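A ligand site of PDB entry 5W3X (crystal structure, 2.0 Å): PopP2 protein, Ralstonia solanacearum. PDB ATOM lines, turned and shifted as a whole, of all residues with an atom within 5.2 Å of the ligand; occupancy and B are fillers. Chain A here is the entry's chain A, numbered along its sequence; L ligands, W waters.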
ATOM      1  N   GLU A  69      -9.789  -5.870 -17.114  1.00  0.00           N
ATOM      2  CA  GLU A  69     -10.964  -5.101 -16.771  1.00  0.00           C
ATOM      3  C   GLU A  69     -11.415  -4.298 -17.977  1.00  0.00           C
ATOM      4  O   GLU A  69     -12.610  -4.089 -18.187  1.00  0.00           O
ATOM      5  CB  GLU A  69     -10.716  -4.196 -15.570  1.00  0.00           C
ATOM      6  CG  GLU A  69     -10.618  -4.941 -14.226  1.00  0.00           C
ATOM      7  CD  GLU A  69     -11.835  -5.853 -13.933  1.00  0.00           C
ATOM      8  OE1 GLU A  69     -11.603  -7.015 -13.531  1.00  0.00           O
ATOM      9  OE2 GLU A  69     -12.991  -5.417 -14.091  1.00  0.00           O
ATOM     10  N   ARG A  72     -13.354  -6.712 -19.992  1.00  0.00           N
ATOM     11  CA  ARG A  72     -14.554  -7.127 -19.284  1.00  0.00           C
ATOM     12  C   ARG A  72     -15.634  -6.039 -19.266  1.00  0.00           C
ATOM     13  O   ARG A  72     -16.823  -6.329 -19.104  1.00  0.00           O
ATOM     14  CB  ARG A  72     -14.145  -7.549 -17.872  1.00  0.00           C
ATOM     15  CG  ARG A  72     -15.248  -8.031 -16.959  1.00  0.00           C
ATOM     16  CD  ARG A  72     -14.664  -8.395 -15.604  1.00  0.00           C
ATOM     17  NE  ARG A  72     -15.659  -8.949 -14.687  1.00  0.00           N
ATOM     18  CZ  ARG A  72     -16.525  -8.209 -13.997  1.00  0.00           C
ATOM     19  NH1 ARG A  72     -17.404  -8.781 -13.179  1.00  0.00           N
ATOM     20  NH2 ARG A  72     -16.510  -6.889 -14.144  1.00  0.00           N
ATOM     21  N   ASN A  73     -15.227  -4.775 -19.454  1.00  0.00           N
ATOM     22  CA  ASN A  73     -16.137  -3.630 -19.436  1.00  0.00           C
ATOM     23  C   ASN A  73     -15.823  -2.657 -20.572  1.00  0.00           C
ATOM     24  O   ASN A  73     -15.086  -1.693 -20.362  1.00  0.00           O
ATOM     25  CB  ASN A  73     -16.065  -2.858 -18.112  1.00  0.00           C
ATOM     26  CG  ASN A  73     -16.212  -3.744 -16.885  1.00  0.00           C
ATOM     27  OD1 ASN A  73     -17.309  -4.155 -16.521  1.00  0.00           O
ATOM     28  ND2 ASN A  73     -15.087  -4.003 -16.199  1.00  0.00           N
ATOM     29  N   SER A 191     -10.585   0.026  -8.251  1.00  0.00           N
ATOM     30  CA  SER A 191     -11.999  -0.120  -7.909  1.00  0.00           C
ATOM     31  C   SER A 191     -12.762   1.198  -8.133  1.00  0.00           C
ATOM     32  O   SER A 191     -13.891   1.202  -8.625  1.00  0.00           O
ATOM     33  CB  SER A 191     -12.173  -0.581  -6.457  1.00  0.00           C
ATOM     34  OG  SER A 191     -13.543  -0.582  -6.089  1.00  0.00           O
ATOM     35  N   LEU A 194     -13.449   1.704 -11.760  1.00  0.00           N
ATOM     36  CA  LEU A 194     -14.587   0.903 -12.189  1.00  0.00           C
ATOM     37  C   LEU A 194     -15.899   1.598 -11.806  1.00  0.00           C
ATOM     38  O   LEU A 194     -16.868   1.605 -12.583  1.00  0.00           O
ATOM     39  CB  LEU A 194     -14.528  -0.488 -11.551  1.00  0.00           C
ATOM     40  CG  LEU A 194     -13.325  -1.324 -11.999  1.00  0.00           C
ATOM     41  CD1 LEU A 194     -13.225  -2.636 -11.208  1.00  0.00           C
ATOM     42  CD2 LEU A 194     -13.415  -1.598 -13.475  1.00  0.00           C
ATOM     43  N   LYS A 195     -15.929   2.178 -10.616  1.00  0.00           N
ATOM     44  CA  LYS A 195     -17.151   2.847 -10.169  1.00  0.00           C
ATOM     45  C   LYS A 195     -17.408   4.138 -10.969  1.00  0.00           C
ATOM     46  O   LYS A 195     -18.553   4.540 -11.163  1.00  0.00           O
ATOM     47  CB  LYS A 195     -17.061   3.174  -8.681  1.00  0.00           C
ATOM     48  CG  LYS A 195     -16.946   1.937  -7.790  1.00  0.00           C
ATOM     49  CD  LYS A 195     -18.023   0.919  -8.109  1.00  0.00           C
ATOM     50  CE  LYS A 195     -17.909  -0.296  -7.189  1.00  0.00           C
ATOM     51  NZ  LYS A 195     -18.703  -1.466  -7.640  1.00  0.00           N
ATOM     52  N   ASP A 198     -19.014   3.108 -13.953  1.00  0.00           N
ATOM     53  CA  ASP A 198     -20.378   2.785 -13.534  1.00  0.00           C
ATOM     54  C   ASP A 198     -21.262   4.047 -13.412  1.00  0.00           C
ATOM     55  O   ASP A 198     -22.443   4.033 -13.749  1.00  0.00           O
ATOM     56  CB  ASP A 198     -20.339   2.016 -12.222  1.00  0.00           C
ATOM     57  CG  ASP A 198     -21.607   1.236 -11.955  1.00  0.00           C
ATOM     58  OD1 ASP A 198     -22.214   0.735 -12.919  1.00  0.00           O
ATOM     59  OD2 ASP A 198     -21.977   1.098 -10.772  1.00  0.00           O
ATOM     60  N   ARG A 244     -21.520   3.445  -2.985  1.00  0.00           N
ATOM     61  CA  ARG A 244     -20.812   2.388  -3.717  1.00  0.00           C
ATOM     62  C   ARG A 244     -19.323   2.671  -3.883  1.00  0.00           C
ATOM     63  O   ARG A 244     -18.546   1.753  -4.080  1.00  0.00           O
ATOM     64  CB  ARG A 244     -21.438   2.146  -5.093  1.00  0.00           C
ATOM     65  CG  ARG A 244     -22.856   1.555  -5.037  1.00  0.00           C
ATOM     66  CD  ARG A 244     -23.226   0.837  -6.334  1.00  0.00           C
ATOM     67  NE  ARG A 244     -22.771  -0.541  -6.334  1.00  0.00           N
ATOM     68  CZ  ARG A 244     -22.175  -1.154  -7.363  1.00  0.00           C
ATOM     69  NH1 ARG A 244     -21.958  -0.482  -8.497  1.00  0.00           N
ATOM     70  NH2 ARG A 244     -21.791  -2.421  -7.250  1.00  0.00           N
ATOM     71  N   LYS A 247     -17.316   1.520  -0.550  1.00  0.00           N
ATOM     72  CA  LYS A 247     -17.453   0.113  -0.114  1.00  0.00           C
ATOM     73  C   LYS A 247     -16.179  -0.515   0.463  1.00  0.00           C
ATOM     74  O   LYS A 247     -16.267  -1.429   1.297  1.00  0.00           O
ATOM     75  CB  LYS A 247     -17.959  -0.761  -1.267  1.00  0.00           C
ATOM     76  CG  LYS A 247     -19.389  -0.433  -1.722  1.00  0.00           C
ATOM     77  CD  LYS A 247     -19.782  -1.220  -2.976  1.00  0.00           C
ATOM     78  CE  LYS A 247     -19.854  -2.726  -2.702  1.00  0.00           C
ATOM     79  NZ  LYS A 247     -20.492  -3.445  -3.845  1.00  0.00           N
ATOM     80  N   HIS A 248     -15.011  -0.032   0.039  1.00  0.00           N
ATOM     81  CA  HIS A 248     -13.766  -0.688   0.470  1.00  0.00           C
ATOM     82  C   HIS A 248     -13.039   0.117   1.532  1.00  0.00           C
ATOM     83  O   HIS A 248     -11.865  -0.144   1.825  1.00  0.00           O
ATOM     84  CB  HIS A 248     -12.848  -0.954  -0.733  1.00  0.00           C
ATOM     85  CG  HIS A 248     -13.475  -1.812  -1.779  1.00  0.00           C
ATOM     86  ND1 HIS A 248     -13.911  -3.093  -1.505  1.00  0.00           N
ATOM     87  CD2 HIS A 248     -13.805  -1.562  -3.070  1.00  0.00           C
ATOM     88  CE1 HIS A 248     -14.455  -3.617  -2.591  1.00  0.00           C
ATOM     89  NE2 HIS A 248     -14.401  -2.702  -3.557  1.00  0.00           N
ATOM     90  N   VAL A 270     -25.765  -1.425  -1.827  1.00  0.00           N
ATOM     91  CA  VAL A 270     -24.499  -1.249  -2.535  1.00  0.00           C
ATOM     92  C   VAL A 270     -24.114  -2.513  -3.304  1.00  0.00           C
ATOM     93  O   VAL A 270     -23.053  -2.573  -3.920  1.00  0.00           O
ATOM     94  CB  VAL A 270     -23.368  -0.859  -1.564  1.00  0.00           C
ATOM     95  CG1 VAL A 270     -23.669   0.488  -0.891  1.00  0.00           C
ATOM     96  CG2 VAL A 270     -23.156  -1.936  -0.513  1.00  0.00           C
ATOM     97  N   ASN A 271     -24.973  -3.519  -3.251  1.00  0.00           N
ATOM     98  CA  ASN A 271     -24.810  -4.739  -4.055  1.00  0.00           C
ATOM     99  C   ASN A 271     -26.140  -5.459  -4.238  1.00  0.00           C
ATOM    100  O   ASN A 271     -27.179  -5.007  -3.748  1.00  0.00           O
ATOM    101  CB  ASN A 271     -23.765  -5.673  -3.442  1.00  0.00           C
ATOM    102  CG  ASN A 271     -24.078  -6.059  -2.002  1.00  0.00           C
ATOM    103  OD1 ASN A 271     -25.238  -6.108  -1.582  1.00  0.00           O
ATOM    104  ND2 ASN A 271     -23.031  -6.354  -1.229  1.00  0.00           N
ATOM    105  N   LYS A 272     -26.104  -6.612  -4.915  1.00  0.00           N
ATOM    106  CA  LYS A 272     -27.319  -7.365  -5.213  1.00  0.00           C
ATOM    107  C   LYS A 272     -27.776  -8.218  -4.032  1.00  0.00           C
ATOM    108  O   LYS A 272     -28.828  -8.867  -4.093  1.00  0.00           O
ATOM    109  CB  LYS A 272     -27.104  -8.238  -6.449  1.00  0.00           C
ATOM    110  CG  LYS A 272     -26.759  -7.437  -7.714  1.00  0.00           C
ATOM    111  CD  LYS A 272     -26.265  -8.355  -8.829  1.00  0.00           C
ATOM    112  CE  LYS A 272     -25.055  -7.739  -9.533  1.00  0.00           C
ATOM    113  NZ  LYS A 272     -24.236  -8.761 -10.247  1.00  0.00           N
ATOM    114  N   ARG A 273     -26.999  -8.225  -2.955  1.00  0.00           N
ATOM    115  CA  ARG A 273     -27.365  -8.907  -1.713  1.00  0.00           C
ATOM    116  C   ARG A 273     -28.220  -7.978  -0.862  1.00  0.00           C
ATOM    117  O   ARG A 273     -28.666  -8.344   0.220  1.00  0.00           O
ATOM    118  CB  ARG A 273     -26.113  -9.336  -0.948  1.00  0.00           C
ATOM    119  CG  ARG A 273     -25.147 -10.198  -1.748  1.00  0.00           C
ATOM    120  CD  ARG A 273     -23.774 -10.235  -1.107  1.00  0.00           C
ATOM    121  NE  ARG A 273     -23.796 -10.860   0.212  1.00  0.00           N
ATOM    122  CZ  ARG A 273     -23.097 -11.937   0.534  1.00  0.00           C
ATOM    123  NH1 ARG A 273     -22.309 -12.513  -0.363  1.00  0.00           N
ATOM    124  NH2 ARG A 273     -23.176 -12.434   1.761  1.00  0.00           N
ATOM    125  N   GLU A 275     -27.333  -5.350   0.769  1.00  0.00           N
ATOM    126  CA  GLU A 275     -26.674  -4.765   1.942  1.00  0.00           C
ATOM    127  C   GLU A 275     -26.542  -3.250   1.782  1.00  0.00           C
ATOM    128  O   GLU A 275     -26.285  -2.760   0.691  1.00  0.00           O
ATOM    129  CB  GLU A 275     -25.283  -5.361   2.153  1.00  0.00           C
ATOM    130  CG  GLU A 275     -25.226  -6.873   2.291  1.00  0.00           C
ATOM    131  CD  GLU A 275     -23.806  -7.369   2.434  1.00  0.00           C
ATOM    132  OE1 GLU A 275     -23.018  -7.181   1.469  1.00  0.00           O
ATOM    133  OE2 GLU A 275     -23.457  -7.925   3.498  1.00  0.00           O
ATOM    134  N   ARG A 280     -22.586  -3.996   4.945  1.00  0.00           N
ATOM    135  CA  ARG A 280     -21.539  -4.676   4.190  1.00  0.00           C
ATOM    136  C   ARG A 280     -20.187  -4.493   4.869  1.00  0.00           C
ATOM    137  O   ARG A 280     -19.413  -5.438   4.991  1.00  0.00           O
ATOM    138  CB  ARG A 280     -21.474  -4.172   2.751  1.00  0.00           C
ATOM    139  CG  ARG A 280     -20.526  -5.019   1.881  1.00  0.00           C
ATOM    140  CD  ARG A 280     -20.294  -4.383   0.507  1.00  0.00           C
ATOM    141  NE  ARG A 280     -19.319  -5.151  -0.254  1.00  0.00           N
ATOM    142  CZ  ARG A 280     -18.000  -5.101  -0.051  1.00  0.00           C
ATOM    143  NH1 ARG A 280     -17.515  -4.314   0.901  1.00  0.00           N
ATOM    144  NH2 ARG A 280     -17.171  -5.826  -0.799  1.00  0.00           N
ATOM    145  N   ARG A 283     -19.909  -6.666   7.972  1.00  0.00           N
ATOM    146  CA  ARG A 283     -19.668  -8.070   7.599  1.00  0.00           C
ATOM    147  C   ARG A 283     -18.181  -8.372   7.310  1.00  0.00           C
ATOM    148  O   ARG A 283     -17.700  -9.464   7.573  1.00  0.00           O
ATOM    149  CB  ARG A 283     -20.520  -8.456   6.384  1.00  0.00           C
ATOM    150  CG  ARG A 283     -20.335  -9.912   5.939  1.00  0.00           C
ATOM    151  CD  ARG A 283     -21.384 -10.325   4.906  1.00  0.00           C
ATOM    152  NE  ARG A 283     -21.360  -9.470   3.714  1.00  0.00           N
ATOM    153  CZ  ARG A 283     -20.603  -9.697   2.647  1.00  0.00           C
ATOM    154  NH1 ARG A 283     -19.757 -10.722   2.640  1.00  0.00           N
ATOM    155  NH2 ARG A 283     -20.661  -8.879   1.599  1.00  0.00           N
ATOM    156  N   LYS A 317     -11.224  -7.935  -2.562  1.00  0.00           N
ATOM    157  CA  LYS A 317     -11.296  -7.338  -3.900  1.00  0.00           C
ATOM    158  C   LYS A 317     -10.089  -7.746  -4.744  1.00  0.00           C
ATOM    159  O   LYS A 317     -10.235  -8.136  -5.894  1.00  0.00           O
ATOM    160  CB  LYS A 317     -11.380  -5.811  -3.821  1.00  0.00           C
ATOM    161  CG  LYS A 317     -11.690  -5.160  -5.177  1.00  0.00           C
ATOM    162  CD  LYS A 317     -13.001  -5.704  -5.718  1.00  0.00           C
ATOM    163  CE  LYS A 317     -13.427  -5.036  -7.000  1.00  0.00           C
ATOM    164  NZ  LYS A 317     -14.737  -5.563  -7.477  1.00  0.00           N
ATOM    165  N   ARG A 324     -10.666 -12.997 -11.834  1.00  0.00           N
ATOM    166  CA  ARG A 324     -11.199 -12.468 -13.083  1.00  0.00           C
ATOM    167  C   ARG A 324     -10.144 -12.408 -14.171  1.00  0.00           C
ATOM    168  O   ARG A 324     -10.389 -12.797 -15.324  1.00  0.00           O
ATOM    169  CB  ARG A 324     -11.801 -11.067 -12.869  1.00  0.00           C
ATOM    170  CG  ARG A 324     -13.291 -11.116 -12.662  1.00  0.00           C
ATOM    171  CD  ARG A 324     -13.842 -10.041 -11.728  1.00  0.00           C
ATOM    172  NE  ARG A 324     -13.564  -8.639 -12.027  1.00  0.00           N
ATOM    173  CZ  ARG A 324     -14.241  -7.654 -11.437  1.00  0.00           C
ATOM    174  NH1 ARG A 324     -13.982  -6.380 -11.693  1.00  0.00           N
ATOM    175  NH2 ARG A 324     -15.199  -7.968 -10.575  1.00  0.00           N
HETATM  176  C1  LIG L   1     -20.364  -7.906  -7.169  1.00  0.00           C
HETATM  177  C2  LIG L   1     -20.016  -7.827  -8.743  1.00  0.00           C
HETATM  178  C3  LIG L   1     -19.487  -6.460  -9.204  1.00  0.00           C
HETATM  179  C4  LIG L   1     -18.073  -6.541  -8.521  1.00  0.00           C
HETATM  180  C5  LIG L   1     -18.115  -6.202  -6.910  1.00  0.00           C
HETATM  181  C6  LIG L   1     -19.277  -7.110  -6.254  1.00  0.00           C
HETATM  182  O1  LIG L   1     -21.622  -7.585  -6.862  1.00  0.00           O
HETATM  183  P1  LIG L   1     -22.793  -8.564  -6.095  1.00  0.00           P
HETATM  184  O2  LIG L   1     -22.503  -8.780  -4.591  1.00  0.00           O
HETATM  185  O3  LIG L   1     -22.936  -9.943  -6.745  1.00  0.00           O
HETATM  186  O4  LIG L   1     -24.148  -7.876  -6.152  1.00  0.00           O
HETATM  187  O5  LIG L   1     -20.996  -8.346  -9.538  1.00  0.00           O
HETATM  188  P2  LIG L   1     -21.151  -9.962  -9.984  1.00  0.00           P
HETATM  189  O6  LIG L   1     -20.095 -10.837  -9.278  1.00  0.00           O
HETATM  190  O7  LIG L   1     -22.535 -10.527  -9.598  1.00  0.00           O
HETATM  191  O8  LIG L   1     -21.029 -10.164 -11.501  1.00  0.00           O
HETATM  192  O9  LIG L   1     -20.248  -5.353  -8.929  1.00  0.00           O
HETATM  193  P3  LIG L   1     -21.410  -4.592 -10.044  1.00  0.00           P
HETATM  194  O10 LIG L   1     -21.881  -3.228  -9.537  1.00  0.00           O
HETATM  195  O11 LIG L   1     -20.794  -4.332 -11.428  1.00  0.00           O
HETATM  196  O12 LIG L   1     -22.641  -5.464 -10.295  1.00  0.00           O
HETATM  197  O13 LIG L   1     -17.091  -5.876  -9.239  1.00  0.00           O
HETATM  198  P4  LIG L   1     -17.216  -4.400 -10.070  1.00  0.00           P
HETATM  199  O14 LIG L   1     -15.874  -3.750 -10.306  1.00  0.00           O
HETATM  200  O15 LIG L   1     -17.978  -4.511 -11.406  1.00  0.00           O
HETATM  201  O16 LIG L   1     -18.032  -3.397  -9.237  1.00  0.00           O
HETATM  202  O17 LIG L   1     -18.240  -4.944  -6.605  1.00  0.00           O
HETATM  203  P5  LIG L   1     -17.468  -3.991  -5.419  1.00  0.00           P
HETATM  204  O18 LIG L   1     -18.247  -2.697  -5.319  1.00  0.00           O
HETATM  205  O19 LIG L   1     -17.483  -4.613  -4.011  1.00  0.00           O
HETATM  206  O20 LIG L   1     -16.003  -3.651  -5.721  1.00  0.00           O
HETATM  207  O21 LIG L   1     -19.894  -6.505  -5.167  1.00  0.00           O
HETATM  208  P6  LIG L   1     -19.705  -6.970  -3.568  1.00  0.00           P
HETATM  209  O22 LIG L   1     -18.231  -6.896  -3.151  1.00  0.00           O
HETATM  210  O23 LIG L   1     -20.517  -6.099  -2.570  1.00  0.00           O
HETATM  211  O24 LIG L   1     -20.193  -8.408  -3.340  1.00  0.00           O
HETATM  212  O   HOH W   1     -20.206  -7.013 -11.896  1.00  0.00           O
HETATM  213  O   HOH W   2     -15.694  -7.971  -7.106  1.00  0.00           O
HETATM  214  O   HOH W   3     -19.261 -10.514  -5.100  1.00  0.00           O
HETATM  215  O   HOH W   4     -15.010  -2.064  -7.902  1.00  0.00           O
HETATM  216  O   HOH W   5     -19.041  -9.247  -1.064  1.00  0.00           O
HETATM  217  O   HOH W   6     -18.622  -1.382 -11.440  1.00  0.00           O
HETATM  218  O   HOH W   7     -20.234  -2.471 -13.026  1.00  0.00           O
HETATM  219  O   HOH W   8     -15.339  -8.361  -4.052  1.00  0.00           O
HETATM  220  O   HOH W   9     -23.460  -5.730  -7.070  1.00  0.00           O
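NH1 of Arg 244 lies within salt-bridge range of OD2 of Asp 198, 2.8 Å away. The guanidinium group (NE) of Arg 244 is in hydrogen-bond range of the backbone carbonyl oxygen (O) of Val 270 (3.2 Å). The guanidinium group (NH1) of Arg 280 is in hydrogen-bond range of the backbone carbonyl oxygen (O) of Lys 247 (3.2 Å). NZ of Lys 247 is in hydrogen-bond range of O of Val 270 (2.7 Å). The backbone NH (N) of Arg 273 lies within hydrogen-bond range of the side-chain amide oxygen (OD1) of Asn 271, at 3.1 Å. OE1 of Glu 275 lies within hydrogen-bond range of ND2 of Asn 271 (2.8 Å). NH1 of Arg 324 is in salt-bridge range of OE2 of Glu 69, 2.8 Å away. The guanidinium group of Arg 72 is in salt-bridge range of the side-chain carboxylate of Glu 69 (3.8 Å).
Residues that only touch the ligand: Leu 194 (3.0 Å), Ser 191 (3.95 Å) and Arg 273 (3.98 Å). Hydrophobic or aromatic side chains within 4 Å of the ligand: Leu 194 and His 248.
The guanidinium group of Arg 244 lies within salt-bridge range of an oxygen (O10) of the ligand (2.4 Å). The backbone NH of Lys 272 is in hydrogen-bond range of an oxygen (O4) of the ligand (2.6 Å). The side-chain amino group (NZ) of Lys 272 is in salt-bridge range of an oxygen (O7) of the ligand (2.5 Å). The side-chain amino group of Lys 195 is in salt-bridge range of an oxygen (O16) of the ligand (2.6 Å). An oxygen (O23) of the ligand is in salt-bridge range of the guanidinium group (NE) of Arg 280 (2.8 Å). An oxygen (O18) of the ligand is in salt-bridge range of the side-chain amino group of Lys 247 (2.8 Å). O20 of the ligand is in hydrogen-bond range of NE2 of His 248, at 2.9 Å. The side-chain amide nitrogen (ND2) of Asn 271 sits at hydrogen-bond distance from an oxygen (O23) of the ligand (2.9 Å). NZ of Lys 317 is in salt-bridge range of O20 of the ligand, at 2.9 Å. The guanidinium group (NH1) of Arg 324 is in salt-bridge range of an oxygen (O14) of the ligand. The guanidinium group (NH2) of Arg 72 lies within salt-bridge range of an oxygen (O15) of the ligand, 3.9 Å away.
Water W5 bridges O24 of the ligand (2.7 Å) and NH2 of Arg 283 (3.1 Å). Water W4 bridges OG of Ser 191 (2.8 Å) and O20 of the ligand (2.9 Å). Water W2 lies within hydrogen-bond range of NZ of Lys 317 and O13 of the ligand.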
